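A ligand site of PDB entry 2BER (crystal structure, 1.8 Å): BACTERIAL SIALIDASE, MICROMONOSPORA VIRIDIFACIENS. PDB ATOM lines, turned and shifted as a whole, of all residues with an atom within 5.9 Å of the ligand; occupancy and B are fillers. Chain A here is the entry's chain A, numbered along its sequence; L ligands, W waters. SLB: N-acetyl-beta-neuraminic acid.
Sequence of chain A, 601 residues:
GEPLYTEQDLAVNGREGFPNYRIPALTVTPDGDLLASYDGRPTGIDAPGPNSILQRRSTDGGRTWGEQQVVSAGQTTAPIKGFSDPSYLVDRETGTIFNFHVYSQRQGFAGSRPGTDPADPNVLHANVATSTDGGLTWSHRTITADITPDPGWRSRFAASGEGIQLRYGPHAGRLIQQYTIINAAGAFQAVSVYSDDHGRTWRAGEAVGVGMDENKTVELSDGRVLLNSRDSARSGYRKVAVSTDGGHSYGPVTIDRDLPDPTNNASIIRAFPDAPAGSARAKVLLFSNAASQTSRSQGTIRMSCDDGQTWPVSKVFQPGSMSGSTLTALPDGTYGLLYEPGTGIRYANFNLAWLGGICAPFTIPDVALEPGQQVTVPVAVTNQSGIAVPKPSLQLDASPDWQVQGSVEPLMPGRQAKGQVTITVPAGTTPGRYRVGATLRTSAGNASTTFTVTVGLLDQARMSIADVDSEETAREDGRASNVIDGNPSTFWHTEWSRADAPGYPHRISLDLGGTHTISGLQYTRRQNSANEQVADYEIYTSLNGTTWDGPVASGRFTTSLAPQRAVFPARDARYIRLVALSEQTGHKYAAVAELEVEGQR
The side-chain carboxylate (OD1) of Asp 85 lies within salt-bridge range of the guanidinium group (NH2) of Arg 41, at 3.6 Å. The guanidinium group of Arg 41 is in salt-bridge range of the side-chain carboxylate of Asp 46 (2.9 Å). The guanidinium group of Arg 41 sits at hydrogen-bond distance from the side-chain hydroxyl of Ser 84. The side-chain carboxylate of Asp 39 is in salt-bridge range of the guanidinium group of Arg 41 (2.9 Å). The guanidinium group (NH2) of Arg 296 sits close to the side-chain amide oxygen (OD1) of Asn 264. The guanidinium group (NH2) of Arg 296 lies within hydrogen-bond range of the backbone carbonyl oxygen (O) of Thr 263 (3.1 Å). O of Arg 22 sits at hydrogen-bond distance from N of Asp 39 (2.8 Å). O of Ser 323 lies within hydrogen-bond range of NH2 of Arg 22 (3.2 Å).
Water W2 lies within hydrogen-bond range of the side-chain amide oxygen (OD1) of Asn 264 (2.7 Å), an oxygen (O2) of the ligand (2.7 Å) and the guanidinium group (NH2) of Arg 22 (2.9 Å). Water W1 bridges O6 of the ligand (2.7 Å) and OD2 of Asp 46 (2.7 Å). Water W4 lies within hydrogen-bond range of O of Ala 47, O10 of the ligand and N of Phe 109. Water W7 lies within hydrogen-bond range of an oxygen (O9) of the ligand (2.9 Å) and the guanidinium group of Arg 230 (3.4 Å). Water W5 lies within hydrogen-bond range of the backbone NH (N) of Ala 47, the side-chain hydroxyl (OG) of Ser 84, an oxygen (O4) of the ligand and the side-chain carboxylate (OD1) of Asp 85. Water W6 lies within hydrogen-bond range of the side-chain carboxylate (OD1) of Asp 46, the guanidinium group (NH1) of Arg 22 and an oxygen (O1B) of the ligand.
Ile 23 touches the ligand. CE2 of Phe 109 touches C9 of the ligand, 3.7 Å away. Phe 157 touches the ligand. Phe 188 touches the ligand (CE2 to O9, 3.8 Å). Hydrophobic or aromatic side chains that line the ligand: Ile 23, Phe 109, Phe 157 and Phe 188. 12 residues have an atom within 4 Å of the ligand: Arg 22, Ile 23, Arg 41, Asp 46, Asp 85, Phe 109, Phe 157, Phe 188, Asp 213, Glu 214, Arg 230 and Arg 296.
The side-chain carboxylate of Asp 213 lies within hydrogen-bond range of an oxygen (O9) of the ligand (2.6 Å). An oxygen (O2) of the ligand sits at hydrogen-bond distance from the side-chain carboxylate (OE2) of Glu 214 (2.7 Å). The side-chain carboxylate of Asp 85 lies within hydrogen-bond range of an oxygen (O4) of the ligand (2.7 Å). O4 of the ligand lies within hydrogen-bond range of NH2 of Arg 41. The guanidinium group (NH2) of Arg 296 is in salt-bridge range of an oxygen (O1A) of the ligand. O1B of the ligand lies within salt-bridge range of NH1 of Arg 22 (3.0 Å). The guanidinium group of Arg 230 is in salt-bridge range of an oxygen (O1A) of the ligand. OD1 of Asp 46 sits close to O4 of the ligand (3.5 Å).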
ATOM      1  N   ARG A  22     -20.280   3.838   0.898  1.00  0.00           N
ATOM      2  CA  ARG A  22     -19.058   3.803   0.121  1.00  0.00           C
ATOM      3  C   ARG A  22     -19.148   4.916  -0.917  1.00  0.00           C
ATOM      4  O   ARG A  22     -20.236   5.441  -1.204  1.00  0.00           O
ATOM      5  CB  ARG A  22     -18.895   2.488  -0.660  1.00  0.00           C
ATOM      6  CG  ARG A  22     -18.723   1.182   0.174  1.00  0.00           C
ATOM      7  CD  ARG A  22     -18.083   0.099  -0.661  1.00  0.00           C
ATOM      8  NE  ARG A  22     -16.774   0.517  -1.154  1.00  0.00           N
ATOM      9  CZ  ARG A  22     -16.290   0.198  -2.352  1.00  0.00           C
ATOM     10  NH1 ARG A  22     -16.981  -0.606  -3.160  1.00  0.00           N
ATOM     11  NH2 ARG A  22     -15.133   0.704  -2.752  1.00  0.00           N
ATOM     12  N   ILE A  23     -18.016   5.184  -1.521  1.00  0.00           N
ATOM     13  CA  ILE A  23     -17.925   5.941  -2.784  1.00  0.00           C
ATOM     14  C   ILE A  23     -17.935   7.471  -2.581  1.00  0.00           C
ATOM     15  O   ILE A  23     -18.940   8.141  -2.834  1.00  0.00           O
ATOM     16  CB  ILE A  23     -18.930   5.505  -3.901  1.00  0.00           C
ATOM     17  CG1 ILE A  23     -19.125   3.961  -3.992  1.00  0.00           C
ATOM     18  CG2 ILE A  23     -18.347   5.957  -5.246  1.00  0.00           C
ATOM     19  CD1 ILE A  23     -17.913   3.137  -4.263  1.00  0.00           C
ATOM     20  N   ASP A  39     -22.535   7.057  -1.444  1.00  0.00           N
ATOM     21  CA  ASP A  39     -23.651   6.096  -1.491  1.00  0.00           C
ATOM     22  C   ASP A  39     -24.101   5.651  -0.088  1.00  0.00           C
ATOM     23  O   ASP A  39     -23.267   5.335   0.775  1.00  0.00           O
ATOM     24  CB  ASP A  39     -23.214   4.788  -2.192  1.00  0.00           C
ATOM     25  CG  ASP A  39     -23.090   4.917  -3.684  1.00  0.00           C
ATOM     26  OD1 ASP A  39     -23.019   6.050  -4.214  1.00  0.00           O
ATOM     27  OD2 ASP A  39     -23.047   3.846  -4.308  1.00  0.00           O
ATOM     28  N   ARG A  41     -26.134   2.267   0.813  1.00  0.00           N
ATOM     29  CA  ARG A  41     -26.323   1.000   0.124  1.00  0.00           C
ATOM     30  C   ARG A  41     -27.173   0.051   0.944  1.00  0.00           C
ATOM     31  O   ARG A  41     -26.636  -0.666   1.811  1.00  0.00           O
ATOM     32  CB  ARG A  41     -24.954   0.367  -0.214  1.00  0.00           C
ATOM     33  CG  ARG A  41     -24.092   1.302  -1.125  1.00  0.00           C
ATOM     34  CD  ARG A  41     -22.848   0.669  -1.686  1.00  0.00           C
ATOM     35  NE  ARG A  41     -22.405   1.354  -2.908  1.00  0.00           N
ATOM     36  CZ  ARG A  41     -21.524   0.850  -3.790  1.00  0.00           C
ATOM     37  NH1 ARG A  41     -20.936  -0.332  -3.591  1.00  0.00           N
ATOM     38  NH2 ARG A  41     -21.256   1.537  -4.902  1.00  0.00           N
ATOM     39  N   ASP A  46     -22.880  -2.511  -5.347  1.00  0.00           N
ATOM     40  CA  ASP A  46     -22.791  -1.512  -6.408  1.00  0.00           C
ATOM     41  C   ASP A  46     -24.161  -1.491  -7.141  1.00  0.00           C
ATOM     42  O   ASP A  46     -25.003  -2.349  -6.935  1.00  0.00           O
ATOM     43  CB  ASP A  46     -21.794  -1.877  -7.481  1.00  0.00           C
ATOM     44  CG  ASP A  46     -20.391  -2.150  -6.989  1.00  0.00           C
ATOM     45  OD1 ASP A  46     -19.936  -1.712  -5.914  1.00  0.00           O
ATOM     46  OD2 ASP A  46     -19.708  -2.813  -7.767  1.00  0.00           O
ATOM     47  N   ALA A  47     -24.339  -0.538  -8.026  1.00  0.00           N
ATOM     48  CA  ALA A  47     -25.487  -0.565  -9.003  1.00  0.00           C
ATOM     49  C   ALA A  47     -25.637  -1.949  -9.609  1.00  0.00           C
ATOM     50  O   ALA A  47     -24.613  -2.511  -9.979  1.00  0.00           O
ATOM     51  CB  ALA A  47     -25.264   0.460 -10.088  1.00  0.00           C
ATOM     52  N   SER A  84     -26.071   6.051  -7.670  1.00  0.00           N
ATOM     53  CA  SER A  84     -24.850   5.510  -7.114  1.00  0.00           C
ATOM     54  C   SER A  84     -23.629   6.156  -7.767  1.00  0.00           C
ATOM     55  O   SER A  84     -23.665   6.506  -8.936  1.00  0.00           O
ATOM     56  CB  SER A  84     -24.853   3.929  -7.253  1.00  0.00           C
ATOM     57  OG  SER A  84     -23.756   3.300  -6.579  1.00  0.00           O
ATOM     58  N   ASP A  85     -22.536   6.265  -7.006  1.00  0.00           N
ATOM     59  CA  ASP A  85     -21.251   6.718  -7.491  1.00  0.00           C
ATOM     60  C   ASP A  85     -21.248   8.241  -7.788  1.00  0.00           C
ATOM     61  O   ASP A  85     -21.234   8.635  -8.960  1.00  0.00           O
ATOM     62  CB  ASP A  85     -20.814   5.946  -8.770  1.00  0.00           C
ATOM     63  CG  ASP A  85     -20.190   4.576  -8.484  1.00  0.00           C
ATOM     64  OD1 ASP A  85     -20.455   4.024  -7.427  1.00  0.00           O
ATOM     65  OD2 ASP A  85     -19.374   4.088  -9.322  1.00  0.00           O
ATOM     66  N   VAL A 102     -24.945   7.473 -11.431  1.00  0.00           N
ATOM     67  CA  VAL A 102     -25.774   6.571 -12.227  1.00  0.00           C
ATOM     68  C   VAL A 102     -27.211   6.617 -11.780  1.00  0.00           C
ATOM     69  O   VAL A 102     -27.530   6.994 -10.644  1.00  0.00           O
ATOM     70  CB  VAL A 102     -25.320   5.070 -12.284  1.00  0.00           C
ATOM     71  CG1 VAL A 102     -23.758   4.987 -12.403  1.00  0.00           C
ATOM     72  CG2 VAL A 102     -25.752   4.352 -11.070  1.00  0.00           C
ATOM     73  N   PHE A 109     -23.421  -1.729 -14.397  1.00  0.00           N
ATOM     74  CA  PHE A 109     -22.410  -1.509 -15.438  1.00  0.00           C
ATOM     75  C   PHE A 109     -22.295  -2.730 -16.337  1.00  0.00           C
ATOM     76  O   PHE A 109     -22.280  -2.600 -17.564  1.00  0.00           O
ATOM     77  CB  PHE A 109     -21.105  -1.181 -14.767  1.00  0.00           C
ATOM     78  CG  PHE A 109     -19.972  -0.893 -15.689  1.00  0.00           C
ATOM     79  CD1 PHE A 109     -20.013   0.201 -16.492  1.00  0.00           C
ATOM     80  CD2 PHE A 109     -18.739  -1.611 -15.594  1.00  0.00           C
ATOM     81  CE1 PHE A 109     -18.955   0.523 -17.323  1.00  0.00           C
ATOM     82  CE2 PHE A 109     -17.682  -1.287 -16.412  1.00  0.00           C
ATOM     83  CZ  PHE A 109     -17.784  -0.200 -17.268  1.00  0.00           C
ATOM     84  N   LEU A 124     -28.108   1.384 -17.943  1.00  0.00           N
ATOM     85  CA  LEU A 124     -27.554   2.143 -16.872  1.00  0.00           C
ATOM     86  C   LEU A 124     -27.446   3.566 -17.405  1.00  0.00           C
ATOM     87  O   LEU A 124     -26.571   3.882 -18.197  1.00  0.00           O
ATOM     88  CB  LEU A 124     -26.173   1.640 -16.441  1.00  0.00           C
ATOM     89  CG  LEU A 124     -25.568   2.324 -15.256  1.00  0.00           C
ATOM     90  CD1 LEU A 124     -26.376   2.142 -14.071  1.00  0.00           C
ATOM     91  CD2 LEU A 124     -24.142   1.897 -14.969  1.00  0.00           C
ATOM     92  N   PHE A 157     -20.472   4.902 -16.730  1.00  0.00           N
ATOM     93  CA  PHE A 157     -20.640   5.562 -15.432  1.00  0.00           C
ATOM     94  C   PHE A 157     -19.627   6.681 -15.242  1.00  0.00           C
ATOM     95  O   PHE A 157     -18.456   6.547 -15.593  1.00  0.00           O
ATOM     96  CB  PHE A 157     -20.678   4.567 -14.282  1.00  0.00           C
ATOM     97  CG  PHE A 157     -19.340   3.890 -13.908  1.00  0.00           C
ATOM     98  CD1 PHE A 157     -18.730   4.201 -12.676  1.00  0.00           C
ATOM     99  CD2 PHE A 157     -18.781   2.879 -14.687  1.00  0.00           C
ATOM    100  CE1 PHE A 157     -17.544   3.532 -12.277  1.00  0.00           C
ATOM    101  CE2 PHE A 157     -17.602   2.223 -14.347  1.00  0.00           C
ATOM    102  CZ  PHE A 157     -16.960   2.548 -13.130  1.00  0.00           C
ATOM    103  N   PHE A 188     -13.369  -1.722 -22.126  1.00  0.00           N
ATOM    104  CA  PHE A 188     -13.643  -0.609 -21.237  1.00  0.00           C
ATOM    105  C   PHE A 188     -12.724   0.530 -21.693  1.00  0.00           C
ATOM    106  O   PHE A 188     -11.466   0.373 -21.735  1.00  0.00           O
ATOM    107  CB  PHE A 188     -13.252  -0.919 -19.793  1.00  0.00           C
ATOM    108  CG  PHE A 188     -14.056  -1.975 -19.106  1.00  0.00           C
ATOM    109  CD1 PHE A 188     -14.950  -2.796 -19.753  1.00  0.00           C
ATOM    110  CD2 PHE A 188     -13.826  -2.210 -17.748  1.00  0.00           C
ATOM    111  CE1 PHE A 188     -15.606  -3.800 -19.034  1.00  0.00           C
ATOM    112  CE2 PHE A 188     -14.520  -3.162 -17.075  1.00  0.00           C
ATOM    113  CZ  PHE A 188     -15.329  -3.972 -17.690  1.00  0.00           C
ATOM    114  N   ASP A 213     -10.857   2.176 -16.823  1.00  0.00           N
ATOM    115  CA  ASP A 213     -11.852   2.068 -15.768  1.00  0.00           C
ATOM    116  C   ASP A 213     -12.026   3.456 -15.147  1.00  0.00           C
ATOM    117  O   ASP A 213     -11.645   4.457 -15.761  1.00  0.00           O
ATOM    118  CB  ASP A 213     -11.467   1.012 -14.719  1.00  0.00           C
ATOM    119  CG  ASP A 213     -12.673   0.375 -14.052  1.00  0.00           C
ATOM    120  OD1 ASP A 213     -13.508   1.120 -13.460  1.00  0.00           O
ATOM    121  OD2 ASP A 213     -12.783  -0.871 -14.110  1.00  0.00           O
ATOM    122  N   GLU A 214     -12.459   3.518 -13.902  1.00  0.00           N
ATOM    123  CA  GLU A 214     -12.610   4.835 -13.249  1.00  0.00           C
ATOM    124  C   GLU A 214     -11.331   5.630 -13.476  1.00  0.00           C
ATOM    125  O   GLU A 214     -10.203   5.181 -13.183  1.00  0.00           O
ATOM    126  CB  GLU A 214     -12.829   4.664 -11.728  1.00  0.00           C
ATOM    127  CG  GLU A 214     -14.107   3.935 -11.303  1.00  0.00           C
ATOM    128  CD  GLU A 214     -14.096   3.392  -9.850  1.00  0.00           C
ATOM    129  OE1 GLU A 214     -12.993   3.008  -9.404  1.00  0.00           O
ATOM    130  OE2 GLU A 214     -15.173   3.327  -9.186  1.00  0.00           O
ATOM    131  N   ARG A 230      -7.634   3.962 -13.320  1.00  0.00           N
ATOM    132  CA  ARG A 230      -7.664   2.602 -12.826  1.00  0.00           C
ATOM    133  C   ARG A 230      -7.467   1.666 -14.018  1.00  0.00           C
ATOM    134  O   ARG A 230      -7.972   1.937 -15.126  1.00  0.00           O
ATOM    135  CB  ARG A 230      -9.006   2.369 -12.133  1.00  0.00           C
ATOM    136  CG  ARG A 230      -9.306   0.928 -11.737  1.00  0.00           C
ATOM    137  CD  ARG A 230     -10.632   0.899 -11.029  1.00  0.00           C
ATOM    138  NE  ARG A 230     -11.212  -0.437 -10.867  1.00  0.00           N
ATOM    139  CZ  ARG A 230     -12.111  -0.740  -9.935  1.00  0.00           C
ATOM    140  NH1 ARG A 230     -12.582   0.210  -9.127  1.00  0.00           N
ATOM    141  NH2 ARG A 230     -12.560  -1.989  -9.806  1.00  0.00           N
ATOM    142  N   SER A 232      -8.323  -1.715 -15.584  1.00  0.00           N
ATOM    143  CA  SER A 232      -9.186  -2.897 -15.454  1.00  0.00           C
ATOM    144  C   SER A 232      -8.459  -4.188 -15.904  1.00  0.00           C
ATOM    145  O   SER A 232      -8.942  -5.273 -15.585  1.00  0.00           O
ATOM    146  CB  SER A 232     -10.539  -2.806 -16.175  1.00  0.00           C
ATOM    147  OG  SER A 232     -10.410  -2.426 -17.538  1.00  0.00           O
ATOM    148  N   THR A 263      -6.050  -1.897  -8.222  1.00  0.00           N
ATOM    149  CA  THR A 263      -7.190  -1.852  -9.181  1.00  0.00           C
ATOM    150  C   THR A 263      -8.355  -1.256  -8.423  1.00  0.00           C
ATOM    151  O   THR A 263      -9.239  -1.961  -7.955  1.00  0.00           O
ATOM    152  CB  THR A 263      -7.546  -3.223  -9.779  1.00  0.00           C
ATOM    153  OG1 THR A 263      -6.311  -3.912 -10.083  1.00  0.00           O
ATOM    154  CG2 THR A 263      -8.434  -3.064 -11.046  1.00  0.00           C
ATOM    155  N   ASN A 264      -8.333   0.064  -8.303  1.00  0.00           N
ATOM    156  CA  ASN A 264      -9.322   0.785  -7.538  1.00  0.00           C
ATOM    157  C   ASN A 264      -9.230   2.256  -7.886  1.00  0.00           C
ATOM    158  O   ASN A 264      -8.350   2.691  -8.616  1.00  0.00           O
ATOM    159  CB  ASN A 264      -9.086   0.659  -6.052  1.00  0.00           C
ATOM    160  CG  ASN A 264     -10.330   0.945  -5.255  1.00  0.00           C
ATOM    161  OD1 ASN A 264     -11.450   0.919  -5.808  1.00  0.00           O
ATOM    162  ND2 ASN A 264     -10.175   1.174  -3.961  1.00  0.00           N
ATOM    163  N   ASN A 265     -10.197   2.992  -7.365  1.00  0.00           N
ATOM    164  CA  ASN A 265     -10.288   4.457  -7.674  1.00  0.00           C
ATOM    165  C   ASN A 265      -9.138   5.203  -6.972  1.00  0.00           C
ATOM    166  O   ASN A 265      -8.473   4.697  -6.056  1.00  0.00           O
ATOM    167  CB  ASN A 265     -11.688   4.999  -7.296  1.00  0.00           C
ATOM    168  CG  ASN A 265     -12.167   6.235  -8.183  1.00  0.00           C
ATOM    169  OD1 ASN A 265     -11.394   6.846  -8.952  1.00  0.00           O
ATOM    170  ND2 ASN A 265     -13.439   6.618  -7.996  1.00  0.00           N
ATOM    171  N   ARG A 296      -6.649  -3.375  -1.020  1.00  0.00           N
ATOM    172  CA  ARG A 296      -7.058  -1.951  -0.791  1.00  0.00           C
ATOM    173  C   ARG A 296      -6.644  -1.514   0.611  1.00  0.00           C
ATOM    174  O   ARG A 296      -7.426  -1.481   1.523  1.00  0.00           O
ATOM    175  CB  ARG A 296      -8.559  -1.813  -1.041  1.00  0.00           C
ATOM    176  CG  ARG A 296      -8.874  -1.983  -2.540  1.00  0.00           C
ATOM    177  CD  ARG A 296     -10.367  -2.018  -2.850  1.00  0.00           C
ATOM    178  NE  ARG A 296     -10.543  -2.285  -4.298  1.00  0.00           N
ATOM    179  CZ  ARG A 296     -11.711  -2.138  -4.914  1.00  0.00           C
ATOM    180  NH1 ARG A 296     -12.763  -1.732  -4.215  1.00  0.00           N
ATOM    181  NH2 ARG A 296     -11.785  -2.335  -6.251  1.00  0.00           N
ATOM    182  N   SER A 323     -10.205   1.888   0.901  1.00  0.00           N
ATOM    183  CA  SER A 323     -10.921   1.413  -0.307  1.00  0.00           C
ATOM    184  C   SER A 323     -11.622   2.475  -1.161  1.00  0.00           C
ATOM    185  O   SER A 323     -12.361   2.156  -2.071  1.00  0.00           O
ATOM    186  CB  SER A 323     -11.928   0.319   0.080  1.00  0.00           C
ATOM    187  OG  SER A 323     -12.770   0.722   1.165  1.00  0.00           O
HETATM  188  C1  SLB L   1     -15.263  -1.117  -6.837  1.00  0.00           C
HETATM  189  C2  SLB L   1     -16.033  -0.058  -7.566  1.00  0.00           C
HETATM  190  C3  SLB L   1     -17.319   0.338  -6.838  1.00  0.00           C
HETATM  191  C4  SLB L   1     -18.216   1.235  -7.710  1.00  0.00           C
HETATM  192  C5  SLB L   1     -18.479   0.469  -9.019  1.00  0.00           C
HETATM  193  C6  SLB L   1     -17.109   0.296  -9.660  1.00  0.00           C
HETATM  194  C7  SLB L   1     -17.192  -0.456 -11.032  1.00  0.00           C
HETATM  195  C8  SLB L   1     -15.864  -0.611 -11.742  1.00  0.00           C
HETATM  196  C9  SLB L   1     -15.989  -1.343 -13.091  1.00  0.00           C
HETATM  197  C10 SLB L   1     -20.224   0.843 -10.628  1.00  0.00           C
HETATM  198  C11 SLB L   1     -21.129   1.822 -11.348  1.00  0.00           C
HETATM  199  N5  SLB L   1     -19.344   1.368  -9.840  1.00  0.00           N
HETATM  200  O1A SLB L   1     -14.415  -1.797  -7.466  1.00  0.00           O
HETATM  201  O1B SLB L   1     -15.441  -1.244  -5.627  1.00  0.00           O
HETATM  202  O2  SLB L   1     -15.090   1.106  -7.660  1.00  0.00           O
HETATM  203  O4  SLB L   1     -19.447   1.546  -7.016  1.00  0.00           O
HETATM  204  O6  SLB L   1     -16.367  -0.613  -8.839  1.00  0.00           O
HETATM  205  O7  SLB L   1     -18.045  -1.618 -10.897  1.00  0.00           O
HETATM  206  O8  SLB L   1     -14.842   0.063 -11.431  1.00  0.00           O
HETATM  207  O9  SLB L   1     -14.863  -2.203 -13.434  1.00  0.00           O
HETATM  208  O10 SLB L   1     -20.400  -0.364 -10.774  1.00  0.00           O
HETATM  209  O   HOH W   1     -17.051  -3.202  -8.318  1.00  0.00           O
HETATM  210  O   HOH W   2     -13.992   1.648  -5.249  1.00  0.00           O
HETATM  211  O   HOH W   3     -18.125  -4.231 -11.358  1.00  0.00           O
HETATM  212  O   HOH W   4     -22.622  -1.757 -11.573  1.00  0.00           O
HETATM  213  O   HOH W   5     -22.448   1.440  -8.298  1.00  0.00           O
HETATM  214  O   HOH W   6     -18.157  -3.236  -4.696  1.00  0.00           O
HETATM  215  O   HOH W   7     -14.318  -4.322 -11.578  1.00  0.00           O
HETATM  216  O   HOH W   8     -17.034  -4.664 -14.441  1.00  0.00           O
